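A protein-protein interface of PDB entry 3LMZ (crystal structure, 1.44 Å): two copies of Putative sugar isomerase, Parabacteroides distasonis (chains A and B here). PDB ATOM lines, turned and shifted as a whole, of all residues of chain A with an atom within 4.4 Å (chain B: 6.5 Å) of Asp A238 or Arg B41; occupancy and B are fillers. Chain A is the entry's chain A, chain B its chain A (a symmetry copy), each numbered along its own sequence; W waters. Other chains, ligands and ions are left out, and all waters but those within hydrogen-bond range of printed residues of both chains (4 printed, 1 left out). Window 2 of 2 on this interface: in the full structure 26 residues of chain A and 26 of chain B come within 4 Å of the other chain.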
ATOM      1  N   GLU A 204      11.132  36.857  21.894  1.00  0.00           N
ATOM      2  CA  GLU A 204      12.339  36.686  22.700  1.00  0.00           C
ATOM      3  C   GLU A 204      13.276  37.853  22.404  1.00  0.00           C
ATOM      4  O   GLU A 204      13.441  38.215  21.257  1.00  0.00           O
ATOM      5  CB  GLU A 204      13.008  35.352  22.329  1.00  0.00           C
ATOM      6  CG  GLU A 204      12.224  34.156  22.753  1.00  0.00           C
ATOM      7  CD  GLU A 204      11.194  33.652  21.742  1.00  0.00           C
ATOM      8  OE1 GLU A 204      10.726  34.390  20.840  1.00  0.00           O
ATOM      9  OE2 GLU A 204      10.779  32.447  21.847  1.00  0.00           O
ATOM     10  N   ARG A 207      15.407  38.654  19.034  1.00  0.00           N
ATOM     11  CA  ARG A 207      14.681  38.226  17.827  1.00  0.00           C
ATOM     12  C   ARG A 207      13.874  39.338  17.187  1.00  0.00           C
ATOM     13  O   ARG A 207      13.411  39.177  16.060  1.00  0.00           O
ATOM     14  CB  ARG A 207      13.770  37.033  18.104  1.00  0.00           C
ATOM     15  CG  ARG A 207      14.480  35.847  18.582  1.00  0.00           C
ATOM     16  CD  ARG A 207      13.551  34.650  18.580  1.00  0.00           C
ATOM     17  NE  ARG A 207      13.997  33.464  19.311  1.00  0.00           N
ATOM     18  CZ  ARG A 207      13.414  32.294  19.232  1.00  0.00           C
ATOM     19  NH1 ARG A 207      12.445  32.084  18.345  1.00  0.00           N
ATOM     20  NH2 ARG A 207      13.865  31.339  19.968  1.00  0.00           N
ATOM     21  N   ASP A 235       3.996  33.107  25.185  1.00  0.00           N
ATOM     22  CA  ASP A 235       3.939  31.768  25.731  1.00  0.00           C
ATOM     23  C   ASP A 235       3.694  31.763  27.259  1.00  0.00           C
ATOM     24  O   ASP A 235       4.347  31.064  28.020  1.00  0.00           O
ATOM     25  CB  ASP A 235       5.224  31.010  25.421  1.00  0.00           C
ATOM     26  CG  ASP A 235       5.403  30.751  23.942  1.00  0.00           C
ATOM     27  OD1 ASP A 235       4.399  30.608  23.187  1.00  0.00           O
ATOM     28  OD2 ASP A 235       6.568  30.682  23.500  1.00  0.00           O
ATOM     29  N   MET A 236       2.798  32.642  27.727  1.00  0.00           N
ATOM     30  CA  MET A 236       2.709  32.931  29.147  1.00  0.00           C
ATOM     31  C   MET A 236       2.236  31.743  30.001  1.00  0.00           C
ATOM     32  O   MET A 236       2.436  31.774  31.210  1.00  0.00           O
ATOM     33  CB  MET A 236       1.817  34.163  29.416  1.00  0.00           C
ATOM     34  CG  MET A 236       2.328  35.420  28.726  1.00  0.00           C
ATOM     35  SD  MET A 236       1.537  37.015  29.389  1.00  0.00           S
ATOM     36  CE  MET A 236       2.625  37.179  30.965  1.00  0.00           C
ATOM     37  N   LYS A 237       1.654  30.697  29.401  1.00  0.00           N
ATOM     38  CA  LYS A 237       1.365  29.467  30.132  1.00  0.00           C
ATOM     39  C   LYS A 237       2.574  28.528  30.284  1.00  0.00           C
ATOM     40  O   LYS A 237       2.515  27.564  31.062  1.00  0.00           O
ATOM     41  CB  LYS A 237       0.212  28.710  29.473  1.00  0.00           C
ATOM     42  CG  LYS A 237      -1.056  29.491  29.503  1.00  0.00           C
ATOM     43  CD  LYS A 237      -2.190  28.792  28.720  1.00  0.00           C
ATOM     44  CE  LYS A 237      -2.159  29.108  27.236  1.00  0.00           C
ATOM     45  NZ  LYS A 237      -2.967  30.356  26.922  1.00  0.00           N
ATOM     46  N   ASP A 238       3.641  28.766  29.517  1.00  0.00           N
ATOM     47  CA  ASP A 238       4.905  27.991  29.599  1.00  0.00           C
ATOM     48  C   ASP A 238       6.076  28.821  29.075  1.00  0.00           C
ATOM     49  O   ASP A 238       6.621  28.520  28.032  1.00  0.00           O
ATOM     50  CB  ASP A 238       4.762  26.642  28.861  1.00  0.00           C
ATOM     51  CG  ASP A 238       5.969  25.738  29.031  1.00  0.00           C
ATOM     52  OD1 ASP A 238       6.800  25.998  29.911  1.00  0.00           O
ATOM     53  OD2 ASP A 238       6.092  24.764  28.236  1.00  0.00           O
ATOM     54  N   PRO A 239       6.412  29.895  29.810  1.00  0.00           N
ATOM     55  CA  PRO A 239       7.296  30.926  29.252  1.00  0.00           C
ATOM     56  C   PRO A 239       8.817  30.721  29.481  1.00  0.00           C
ATOM     57  O   PRO A 239       9.660  31.560  29.094  1.00  0.00           O
ATOM     58  CB  PRO A 239       6.826  32.164  30.018  1.00  0.00           C
ATOM     59  CG  PRO A 239       6.470  31.636  31.404  1.00  0.00           C
ATOM     60  CD  PRO A 239       5.746  30.355  31.067  1.00  0.00           C
ATOM     61  N   PHE A 240       9.144  29.656  30.239  1.00  0.00           N
ATOM     62  CA  PHE A 240      10.464  29.510  30.836  1.00  0.00           C
ATOM     63  C   PHE A 240      11.574  29.571  29.762  1.00  0.00           C
ATOM     64  O   PHE A 240      12.604  30.294  29.942  1.00  0.00           O
ATOM     65  CB  PHE A 240      10.537  28.234  31.673  1.00  0.00           C
ATOM     66  CG  PHE A 240       9.548  28.258  32.786  1.00  0.00           C
ATOM     67  CD1 PHE A 240       9.819  28.923  33.963  1.00  0.00           C
ATOM     68  CD2 PHE A 240       8.294  27.679  32.615  1.00  0.00           C
ATOM     69  CE1 PHE A 240       8.842  28.983  34.960  1.00  0.00           C
ATOM     70  CE2 PHE A 240       7.318  27.749  33.602  1.00  0.00           C
ATOM     71  CZ  PHE A 240       7.611  28.378  34.784  1.00  0.00           C
ATOM     72  N   LEU A 241      11.395  28.838  28.679  1.00  0.00           N
ATOM     73  CA  LEU A 241      12.406  28.806  27.648  1.00  0.00           C
ATOM     74  C   LEU A 241      12.673  30.187  27.027  1.00  0.00           C
ATOM     75  O   LEU A 241      13.804  30.562  26.740  1.00  0.00           O
ATOM     76  CB  LEU A 241      12.025  27.764  26.579  1.00  0.00           C
ATOM     77  CG  LEU A 241      13.148  27.106  25.791  1.00  0.00           C
ATOM     78  CD1 LEU A 241      13.907  26.044  26.596  1.00  0.00           C
ATOM     79  CD2 LEU A 241      12.498  26.528  24.555  1.00  0.00           C
ATOM     80  N   LEU B  36      13.167  17.776  19.811  1.00  0.00           N
ATOM     81  CA  LEU B  36      12.833  18.544  18.602  1.00  0.00           C
ATOM     82  C   LEU B  36      11.943  19.752  18.953  1.00  0.00           C
ATOM     83  O   LEU B  36      12.123  20.816  18.387  1.00  0.00           O
ATOM     84  CB  LEU B  36      12.172  17.642  17.554  1.00  0.00           C
ATOM     85  CG  LEU B  36      13.068  16.569  16.956  1.00  0.00           C
ATOM     86  CD1 LEU B  36      12.206  15.653  16.059  1.00  0.00           C
ATOM     87  CD2 LEU B  36      14.240  17.162  16.222  1.00  0.00           C
ATOM     88  N   LYS B  37      11.001  19.595  19.847  1.00  0.00           N
ATOM     89  CA  LYS B  37      10.158  20.696  20.249  1.00  0.00           C
ATOM     90  C   LYS B  37      10.997  21.832  20.885  1.00  0.00           C
ATOM     91  O   LYS B  37      10.768  23.035  20.647  1.00  0.00           O
ATOM     92  CB  LYS B  37       9.062  20.183  21.183  1.00  0.00           C
ATOM     93  CG  LYS B  37       7.959  19.504  20.362  1.00  0.00           C
ATOM     94  CD  LYS B  37       6.896  18.755  21.207  1.00  0.00           C
ATOM     95  CE  LYS B  37       5.863  18.017  20.291  1.00  0.00           C
ATOM     96  NZ  LYS B  37       5.045  17.032  21.101  1.00  0.00           N
ATOM     97  N   THR B  38      11.994  21.445  21.700  1.00  0.00           N
ATOM     98  CA  THR B  38      12.836  22.412  22.311  1.00  0.00           C
ATOM     99  C   THR B  38      13.655  23.125  21.262  1.00  0.00           C
ATOM    100  O   THR B  38      13.760  24.364  21.291  1.00  0.00           O
ATOM    101  CB  THR B  38      13.709  21.776  23.416  1.00  0.00           C
ATOM    102  OG1 THR B  38      12.880  21.038  24.316  1.00  0.00           O
ATOM    103  CG2 THR B  38      14.560  22.787  24.124  1.00  0.00           C
ATOM    104  N   LEU B  39      14.308  22.405  20.345  1.00  0.00           N
ATOM    105  CA  LEU B  39      15.059  23.091  19.280  1.00  0.00           C
ATOM    106  C   LEU B  39      14.163  24.051  18.486  1.00  0.00           C
ATOM    107  O   LEU B  39      14.581  25.147  18.129  1.00  0.00           O
ATOM    108  CB  LEU B  39      15.725  22.086  18.292  1.00  0.00           C
ATOM    109  CG  LEU B  39      17.116  21.545  18.688  1.00  0.00           C
ATOM    110  CD1 LEU B  39      17.116  20.829  20.002  1.00  0.00           C
ATOM    111  CD2 LEU B  39      17.603  20.633  17.570  1.00  0.00           C
ATOM    112  N   GLU B  40      12.985  23.592  18.135  1.00  0.00           N
ATOM    113  CA  GLU B  40      12.031  24.383  17.359  1.00  0.00           C
ATOM    114  C   GLU B  40      11.765  25.730  18.069  1.00  0.00           C
ATOM    115  O   GLU B  40      11.792  26.791  17.471  1.00  0.00           O
ATOM    116  CB  GLU B  40      10.721  23.618  17.134  1.00  0.00           C
ATOM    117  CG  GLU B  40       9.714  24.242  16.258  1.00  0.00           C
ATOM    118  CD  GLU B  40       8.575  23.277  15.980  1.00  0.00           C
ATOM    119  OE1 GLU B  40       8.179  22.524  16.890  1.00  0.00           O
ATOM    120  OE2 GLU B  40       8.019  23.285  14.855  1.00  0.00           O
ATOM    121  N   ARG B  41      11.483  25.666  19.373  1.00  0.00           N
ATOM    122  CA  ARG B  41      11.172  26.861  20.173  1.00  0.00           C
ATOM    123  C   ARG B  41      12.420  27.792  20.271  1.00  0.00           C
ATOM    124  O   ARG B  41      12.251  28.978  20.352  1.00  0.00           O
ATOM    125  CB  ARG B  41      10.672  26.473  21.582  1.00  0.00           C
ATOM    126  CG  ARG B  41       9.297  25.857  21.631  1.00  0.00           C
ATOM    127  CD  ARG B  41       8.824  25.707  23.102  1.00  0.00           C
ATOM    128  NE  ARG B  41       8.546  27.013  23.702  1.00  0.00           N
ATOM    129  CZ  ARG B  41       8.381  27.231  25.006  1.00  0.00           C
ATOM    130  NH1 ARG B  41       8.439  26.225  25.849  1.00  0.00           N
ATOM    131  NH2 ARG B  41       8.143  28.437  25.477  1.00  0.00           N
ATOM    132  N   LEU B  42      13.614  27.198  20.288  1.00  0.00           N
ATOM    133  CA  LEU B  42      14.859  27.966  20.296  1.00  0.00           C
ATOM    134  C   LEU B  42      15.354  28.451  18.956  1.00  0.00           C
ATOM    135  O   LEU B  42      16.358  29.120  18.877  1.00  0.00           O
ATOM    136  CB  LEU B  42      15.987  27.162  20.938  1.00  0.00           C
ATOM    137  CG  LEU B  42      15.837  26.763  22.383  1.00  0.00           C
ATOM    138  CD1 LEU B  42      16.860  25.625  22.702  1.00  0.00           C
ATOM    139  CD2 LEU B  42      16.009  27.967  23.260  1.00  0.00           C
ATOM    140  N   ASP B  43      14.610  28.178  17.880  1.00  0.00           N
ATOM    141  CA  ASP B  43      15.028  28.535  16.515  1.00  0.00           C
ATOM    142  C   ASP B  43      16.353  27.908  16.107  1.00  0.00           C
ATOM    143  O   ASP B  43      17.163  28.508  15.412  1.00  0.00           O
ATOM    144  CB  ASP B  43      15.047  30.049  16.331  1.00  0.00           C
ATOM    145  CG  ASP B  43      15.091  30.507  14.859  1.00  0.00           C
ATOM    146  OD1 ASP B  43      14.514  29.821  13.972  1.00  0.00           O
ATOM    147  OD2 ASP B  43      15.716  31.574  14.576  1.00  0.00           O
ATOM    148  N   ILE B  44      16.551  26.646  16.489  1.00  0.00           N
ATOM    149  CA  ILE B  44      17.752  25.876  16.181  1.00  0.00           C
ATOM    150  C   ILE B  44      17.350  24.796  15.164  1.00  0.00           C
ATOM    151  O   ILE B  44      16.355  24.091  15.374  1.00  0.00           O
ATOM    152  CB  ILE B  44      18.387  25.225  17.464  1.00  0.00           C
ATOM    153  CG1 ILE B  44      18.872  26.344  18.414  1.00  0.00           C
ATOM    154  CG2 ILE B  44      19.473  24.200  17.085  1.00  0.00           C
ATOM    155  CD1 ILE B  44      19.369  25.865  19.798  1.00  0.00           C
ATOM    156  N   LYS B 251      23.760  33.522  20.856  1.00  0.00           N
ATOM    157  CA  LYS B 251      23.188  34.235  19.711  1.00  0.00           C
ATOM    158  C   LYS B 251      23.667  35.710  19.711  1.00  0.00           C
ATOM    159  O   LYS B 251      24.049  36.274  18.690  1.00  0.00           O
ATOM    160  CB  LYS B 251      21.666  34.199  19.716  1.00  0.00           C
ATOM    161  CG  LYS B 251      21.049  32.874  19.275  1.00  0.00           C
ATOM    162  CD  LYS B 251      19.514  32.938  19.402  1.00  0.00           C
ATOM    163  CE  LYS B 251      18.819  31.692  18.913  1.00  0.00           C
ATOM    164  NZ  LYS B 251      17.303  31.829  18.988  1.00  0.00           N
HETATM  165  O   HOH W   1      11.142  29.636  17.303  1.00  0.00           O
HETATM  166  O   HOH W   2       7.769  29.141  21.695  1.00  0.00           O
HETATM  167  O   HOH W   3       9.801  30.488  20.230  1.00  0.00           O
HETATM  168  O   HOH W   4       8.759  31.625  24.728  1.00  0.00           O
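NE of Arg A207 lies within salt-bridge range of OE1 of Glu A204 (3.7 Å).
The backbone carbonyl oxygen of Leu B42 is in hydrogen-bond range of the side-chain amino group of Lys B251 (2.9 Å).
C of Leu B42 touches NH2 of Arg A207 (3.4 Å).
NH2 of Arg A207 touches N of Asp B43, at 3.9 Å.
NZ of Lys B251 touches NH2 of Arg A207, 3.6 Å away.
Leu A241 touches Arg B41.
CG of Leu A241 touches CD2 of Leu B42, at 3.9 Å.
Water W2 bridges OD2 of Asp A235 (2.7 Å) and NE of Arg B41 (3.0 Å).
Water W4 lies within hydrogen-bond range of OD2 of Asp A235 (2.7 Å) and NH2 of Arg B41 (3.3 Å).
Water W3 bridges the side-chain carboxylate (OE2) of Glu A204 (2.7 Å) and the backbone carbonyl oxygen (O) of Arg B41 (2.9 Å).
Water W1 lies within hydrogen-bond range of the backbone carbonyl oxygen (O) of Glu B40 (2.9 Å), the guanidinium group (NH1) of Arg A207 (3.0 Å) and the backbone carbonyl oxygen (O) of Arg B41 (3.3 Å).
The backbone carbonyl oxygen (O) of Arg B41 is in hydrogen-bond range of the guanidinium group (NH2) of Arg A207 (2.9 Å).
The guanidinium group of Arg B41 is in salt-bridge range of the side-chain carboxylate of Asp A235, at 3.4 Å.
NH1 of Arg B41 lies within salt-bridge range of OD2 of Asp A238 (3.7 Å).
Asp A238 touches just one residue of chain B: Arg B41 (3.0 Å).
Printed residues of chain A within 4 Å of Arg B41: Arg A207 (2.9 Å), Asp A235 (3.4 Å), Asp A238 (3.0 Å) and Leu A241 (3.5 Å).
Of the printed residues of chain A, Leu B42 touches Arg A207 and Leu A241.
Of the printed residues of chain A, Asp B43 touches Arg A207 (3.9 Å).
Printed residues of chain B within 4 Å of Leu A241: Arg B41 (3.5 Å) and Leu B42 (3.9 Å).
Of the printed residues of chain A, Lys B251 touches Arg A207 (3.6 Å).
Of the printed residues of chain B, Arg A207 touches Arg B41 (2.9 Å), Leu B42 (3.4 Å), Asp B43 (3.9 Å) and Lys B251 (3.6 Å).
The nearest printed residue of chain A that does not touch Leu B42 is Glu A204 (6.2 Å).
Hydrophobic or aromatic side chains of chain A within 4 Å of the printed part of chain B: Leu A241.
Hydrophobic or aromatic side chains of chain B within 4 Å of the printed part of chain A: Leu B42.
No position is printed for both chains.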
